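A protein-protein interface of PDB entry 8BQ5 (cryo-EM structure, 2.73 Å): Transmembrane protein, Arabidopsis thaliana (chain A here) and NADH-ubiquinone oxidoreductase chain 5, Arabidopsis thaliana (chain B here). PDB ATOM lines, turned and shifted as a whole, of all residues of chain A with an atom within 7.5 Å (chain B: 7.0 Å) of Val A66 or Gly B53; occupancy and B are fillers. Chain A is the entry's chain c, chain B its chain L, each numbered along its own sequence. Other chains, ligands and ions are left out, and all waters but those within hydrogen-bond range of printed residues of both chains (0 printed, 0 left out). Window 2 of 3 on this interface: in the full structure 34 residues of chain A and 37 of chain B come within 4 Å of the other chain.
The backbone carbonyl oxygen (O) of Leu B52 is in hydrogen-bond range of the guanidinium group (NH1) of Arg A67 (3.5 Å).
O of Gly B53 is in hydrogen-bond range of N of Val A66 (3.3 Å).
The side-chain hydroxyl (OG) of Ser B55 lies within hydrogen-bond range of the backbone carbonyl oxygen (O) of His A63 (2.8 Å).
N of Leu B52 lies within hydrogen-bond range of O of Phe B47 (3.5 Å).
O of Glu B49 is in hydrogen-bond range of N of Ser B55.
O of Tyr B48 sits at hydrogen-bond distance from N of Gly B53 (2.9 Å).
The backbone NH of Ser B55 lies within hydrogen-bond range of the backbone carbonyl oxygen of Val B50, 3.4 Å away.
CA of Pro A65 touches O of Gly B53, at 3.6 Å.
CB of Ser B55 touches CB of Pro A65, 3.9 Å away.
Tyr B48 touches Arg A67 (OH to CD, 3.4 Å).
Arg A67 touches Gly B53.
Ile A69 touches Glu B49.
Pro A68 touches none of the printed residues of chain B.
Printed residues of chain B within 4 Å of Ile A69: Glu B49.
Of the printed residues of chain A, Glu B49 touches Ile A69.
Val B50 touches none of the printed residues of chain A.
Printed residues of chain A within 4 Å of Gly B53: Pro A65 (3.6 Å), Val A66 (3.3 Å) and Arg A67 (3.8 Å).
No residue of chain A comes within 4 Å of Ala B54.
Printed residues of chain A within 4 Å of Ser B55: His A63 (2.8 Å) and Pro A65 (3.9 Å).
The nearest printed residue of chain B that does not touch Val A66 is Leu B52 (4.3 Å).
The nearest residue of chain A that does not touch Gly B53 is Met A64 (5.0 Å).
Hydrophobic or aromatic side chains of chain A within 4 Å of the printed part of chain B: Pro A65, Val A66 and Ile A69.
Of the 10 printed residues of chain B, 5 touch a printed residue of chain A.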
ATOM      1  N   HIS A  63      13.675 -24.948 -23.712  1.00  0.00           N
ATOM      2  CA  HIS A  63      13.748 -24.210 -22.459  1.00  0.00           C
ATOM      3  C   HIS A  63      13.746 -25.179 -21.288  1.00  0.00           C
ATOM      4  O   HIS A  63      12.903 -26.080 -21.225  1.00  0.00           O
ATOM      5  CB  HIS A  63      12.572 -23.241 -22.336  1.00  0.00           C
ATOM      6  CG  HIS A  63      12.584 -22.150 -23.358  1.00  0.00           C
ATOM      7  ND1 HIS A  63      11.463 -21.787 -24.072  1.00  0.00           N
ATOM      8  CD2 HIS A  63      13.584 -21.351 -23.797  1.00  0.00           C
ATOM      9  CE1 HIS A  63      11.770 -20.807 -24.902  1.00  0.00           C
ATOM     10  NE2 HIS A  63      13.052 -20.524 -24.754  1.00  0.00           N
ATOM     11  N   MET A  64      14.684 -24.991 -20.366  1.00  0.00           N
ATOM     12  CA  MET A  64      14.681 -25.771 -19.138  1.00  0.00           C
ATOM     13  C   MET A  64      13.457 -25.400 -18.305  1.00  0.00           C
ATOM     14  O   MET A  64      13.172 -24.207 -18.129  1.00  0.00           O
ATOM     15  CB  MET A  64      15.955 -25.526 -18.330  1.00  0.00           C
ATOM     16  CG  MET A  64      17.239 -25.954 -19.018  1.00  0.00           C
ATOM     17  SD  MET A  64      17.334 -27.728 -19.310  1.00  0.00           S
ATOM     18  CE  MET A  64      18.933 -27.847 -20.109  1.00  0.00           C
ATOM     19  N   PRO A  65      12.715 -26.372 -17.785  1.00  0.00           N
ATOM     20  CA  PRO A  65      11.525 -26.047 -16.995  1.00  0.00           C
ATOM     21  C   PRO A  65      11.891 -25.412 -15.662  1.00  0.00           C
ATOM     22  O   PRO A  65      12.989 -25.594 -15.130  1.00  0.00           O
ATOM     23  CB  PRO A  65      10.851 -27.408 -16.799  1.00  0.00           C
ATOM     24  CG  PRO A  65      11.976 -28.383 -16.859  1.00  0.00           C
ATOM     25  CD  PRO A  65      12.958 -27.824 -17.852  1.00  0.00           C
ATOM     26  N   VAL A  66      10.940 -24.642 -15.128  1.00  0.00           N
ATOM     27  CA  VAL A  66      11.163 -23.973 -13.849  1.00  0.00           C
ATOM     28  C   VAL A  66      11.317 -24.992 -12.726  1.00  0.00           C
ATOM     29  O   VAL A  66      11.965 -24.719 -11.709  1.00  0.00           O
ATOM     30  CB  VAL A  66      10.032 -22.966 -13.564  1.00  0.00           C
ATOM     31  CG1 VAL A  66       9.707 -22.165 -14.814  1.00  0.00           C
ATOM     32  CG2 VAL A  66       8.788 -23.671 -13.039  1.00  0.00           C
ATOM     33  N   ARG A  67      10.734 -26.172 -12.882  1.00  0.00           N
ATOM     34  CA  ARG A  67      10.845 -27.244 -11.907  1.00  0.00           C
ATOM     35  C   ARG A  67      11.116 -28.554 -12.627  1.00  0.00           C
ATOM     36  O   ARG A  67      10.865 -28.672 -13.831  1.00  0.00           O
ATOM     37  CB  ARG A  67       9.571 -27.369 -11.055  1.00  0.00           C
ATOM     38  CG  ARG A  67       8.277 -27.388 -11.840  1.00  0.00           C
ATOM     39  CD  ARG A  67       7.092 -27.505 -10.901  1.00  0.00           C
ATOM     40  NE  ARG A  67       6.745 -26.228 -10.290  1.00  0.00           N
ATOM     41  CZ  ARG A  67       6.049 -25.274 -10.890  1.00  0.00           C
ATOM     42  NH1 ARG A  67       5.610 -25.413 -12.130  1.00  0.00           N
ATOM     43  NH2 ARG A  67       5.782 -24.151 -10.228  1.00  0.00           N
ATOM     44  N   PRO A  68      11.652 -29.553 -11.925  1.00  0.00           N
ATOM     45  CA  PRO A  68      11.867 -30.859 -12.557  1.00  0.00           C
ATOM     46  C   PRO A  68      10.559 -31.469 -13.042  1.00  0.00           C
ATOM     47  O   PRO A  68       9.507 -31.312 -12.419  1.00  0.00           O
ATOM     48  CB  PRO A  68      12.502 -31.696 -11.439  1.00  0.00           C
ATOM     49  CG  PRO A  68      12.172 -30.963 -10.169  1.00  0.00           C
ATOM     50  CD  PRO A  68      12.181 -29.521 -10.551  1.00  0.00           C
ATOM     51  N   ILE A  69      10.625 -32.179 -14.173  1.00  0.00           N
ATOM     52  CA  ILE A  69       9.376 -32.742 -14.771  1.00  0.00           C
ATOM     53  C   ILE A  69       9.559 -34.228 -15.062  1.00  0.00           C
ATOM     54  O   ILE A  69      10.705 -34.658 -15.257  1.00  0.00           O
ATOM     55  CB  ILE A  69       8.983 -31.962 -16.041  1.00  0.00           C
ATOM     56  CG1 ILE A  69      10.153 -31.798 -17.013  1.00  0.00           C
ATOM     57  CG2 ILE A  69       8.363 -30.619 -15.681  1.00  0.00           C
ATOM     58  CD1 ILE A  69       9.809 -30.984 -18.235  1.00  0.00           C
ATOM     59  N   GLN A  72      12.171 -35.073 -17.690  1.00  0.00           N
ATOM     60  CA  GLN A  72      13.633 -34.858 -17.491  1.00  0.00           C
ATOM     61  C   GLN A  72      14.302 -36.202 -17.176  1.00  0.00           C
ATOM     62  O   GLN A  72      15.529 -36.206 -16.972  1.00  0.00           O
ATOM     63  CB  GLN A  72      13.899 -33.809 -16.412  1.00  0.00           C
ATOM     64  CG  GLN A  72      13.823 -32.383 -16.932  1.00  0.00           C
ATOM     65  CD  GLN A  72      14.412 -31.384 -15.970  1.00  0.00           C
ATOM     66  OE1 GLN A  72      14.312 -31.530 -14.754  1.00  0.00           O
ATOM     67  NE2 GLN A  72      15.034 -30.352 -16.513  1.00  0.00           N
ATOM     68  N   PHE B  47       0.276 -30.795 -19.606  1.00  0.00           N
ATOM     69  CA  PHE B  47      -0.102 -29.472 -19.127  1.00  0.00           C
ATOM     70  C   PHE B  47       0.810 -29.025 -17.991  1.00  0.00           C
ATOM     71  O   PHE B  47       1.157 -27.843 -17.887  1.00  0.00           O
ATOM     72  CB  PHE B  47      -1.563 -29.489 -18.682  1.00  0.00           C
ATOM     73  CG  PHE B  47      -2.080 -28.155 -18.238  1.00  0.00           C
ATOM     74  CD1 PHE B  47      -2.516 -27.224 -19.161  1.00  0.00           C
ATOM     75  CD2 PHE B  47      -2.136 -27.838 -16.893  1.00  0.00           C
ATOM     76  CE1 PHE B  47      -2.998 -25.998 -18.750  1.00  0.00           C
ATOM     77  CE2 PHE B  47      -2.614 -26.615 -16.477  1.00  0.00           C
ATOM     78  CZ  PHE B  47      -3.046 -25.694 -17.406  1.00  0.00           C
ATOM     79  N   TYR B  48       1.203 -29.961 -17.125  1.00  0.00           N
ATOM     80  CA  TYR B  48       2.160 -29.657 -16.067  1.00  0.00           C
ATOM     81  C   TYR B  48       3.504 -29.224 -16.640  1.00  0.00           C
ATOM     82  O   TYR B  48       4.066 -28.202 -16.227  1.00  0.00           O
ATOM     83  CB  TYR B  48       2.333 -30.887 -15.177  1.00  0.00           C
ATOM     84  CG  TYR B  48       3.016 -30.634 -13.859  1.00  0.00           C
ATOM     85  CD1 TYR B  48       2.455 -29.793 -12.911  1.00  0.00           C
ATOM     86  CD2 TYR B  48       4.228 -31.239 -13.562  1.00  0.00           C
ATOM     87  CE1 TYR B  48       3.075 -29.572 -11.707  1.00  0.00           C
ATOM     88  CE2 TYR B  48       4.860 -31.016 -12.358  1.00  0.00           C
ATOM     89  CZ  TYR B  48       4.280 -30.179 -11.435  1.00  0.00           C
ATOM     90  OH  TYR B  48       4.905 -29.955 -10.231  1.00  0.00           O
ATOM     91  N   GLU B  49       4.043 -29.957 -17.599  1.00  0.00           N
ATOM     92  CA  GLU B  49       5.412 -29.616 -18.060  1.00  0.00           C
ATOM     93  C   GLU B  49       5.414 -28.393 -18.978  1.00  0.00           C
ATOM     94  O   GLU B  49       6.436 -27.683 -18.977  1.00  0.00           O
ATOM     95  CB  GLU B  49       6.004 -30.813 -18.796  1.00  0.00           C
ATOM     96  CG  GLU B  49       5.852 -32.131 -18.063  1.00  0.00           C
ATOM     97  CD  GLU B  49       6.508 -33.292 -18.785  1.00  0.00           C
ATOM     98  OE1 GLU B  49       6.961 -33.092 -19.927  1.00  0.00           O
ATOM     99  OE2 GLU B  49       6.570 -34.390 -18.204  1.00  0.00           O
ATOM    100  N   VAL B  50       4.318 -28.111 -19.684  1.00  0.00           N
ATOM    101  CA  VAL B  50       4.343 -27.045 -20.735  1.00  0.00           C
ATOM    102  C   VAL B  50       3.722 -25.733 -20.255  1.00  0.00           C
ATOM    103  O   VAL B  50       4.264 -24.675 -20.606  1.00  0.00           O
ATOM    104  CB  VAL B  50       3.648 -27.544 -22.023  1.00  0.00           C
ATOM    105  CG1 VAL B  50       3.569 -26.466 -23.090  1.00  0.00           C
ATOM    106  CG2 VAL B  50       4.314 -28.788 -22.586  1.00  0.00           C
ATOM    107  N   ALA B  51       2.643 -25.796 -19.480  1.00  0.00           N
ATOM    108  CA  ALA B  51       1.931 -24.554 -19.109  1.00  0.00           C
ATOM    109  C   ALA B  51       2.415 -23.999 -17.763  1.00  0.00           C
ATOM    110  O   ALA B  51       2.816 -22.827 -17.729  1.00  0.00           O
ATOM    111  CB  ALA B  51       0.458 -24.845 -19.091  1.00  0.00           C
ATOM    112  N   LEU B  52       2.323 -24.795 -16.695  1.00  0.00           N
ATOM    113  CA  LEU B  52       2.798 -24.349 -15.359  1.00  0.00           C
ATOM    114  C   LEU B  52       4.330 -24.361 -15.351  1.00  0.00           C
ATOM    115  O   LEU B  52       4.922 -23.371 -14.886  1.00  0.00           O
ATOM    116  CB  LEU B  52       2.216 -25.275 -14.289  1.00  0.00           C
ATOM    117  CG  LEU B  52       0.711 -25.515 -14.400  1.00  0.00           C
ATOM    118  CD1 LEU B  52       0.250 -26.583 -13.424  1.00  0.00           C
ATOM    119  CD2 LEU B  52      -0.063 -24.225 -14.192  1.00  0.00           C
ATOM    120  N   GLY B  53       4.940 -25.425 -15.866  1.00  0.00           N
ATOM    121  CA  GLY B  53       6.413 -25.543 -15.927  1.00  0.00           C
ATOM    122  C   GLY B  53       7.027 -24.661 -16.996  1.00  0.00           C
ATOM    123  O   GLY B  53       8.267 -24.579 -17.027  1.00  0.00           O
ATOM    124  N   ALA B  54       6.208 -24.063 -17.865  1.00  0.00           N
ATOM    125  CA  ALA B  54       6.695 -23.119 -18.906  1.00  0.00           C
ATOM    126  C   ALA B  54       7.803 -23.741 -19.762  1.00  0.00           C
ATOM    127  O   ALA B  54       8.806 -23.046 -20.001  1.00  0.00           O
ATOM    128  CB  ALA B  54       7.155 -21.832 -18.262  1.00  0.00           C
ATOM    129  N   SER B  55       7.641 -24.991 -20.192  1.00  0.00           N
ATOM    130  CA  SER B  55       8.627 -25.643 -21.099  1.00  0.00           C
ATOM    131  C   SER B  55       7.881 -26.251 -22.290  1.00  0.00           C
ATOM    132  O   SER B  55       7.235 -27.288 -22.096  1.00  0.00           O
ATOM    133  CB  SER B  55       9.446 -26.674 -20.373  1.00  0.00           C
ATOM    134  OG  SER B  55      10.349 -27.323 -21.256  1.00  0.00           O
ATOM    135  N   ALA B  56       8.003 -25.649 -23.477  1.00  0.00           N
ATOM    136  CA  ALA B  56       7.251 -26.103 -24.670  1.00  0.00           C
ATOM    137  C   ALA B  56       7.915 -27.318 -25.323  1.00  0.00           C
ATOM    138  O   ALA B  56       9.127 -27.509 -25.121  1.00  0.00           O
ATOM    139  CB  ALA B  56       7.118 -24.949 -25.632  1.00  0.00           C
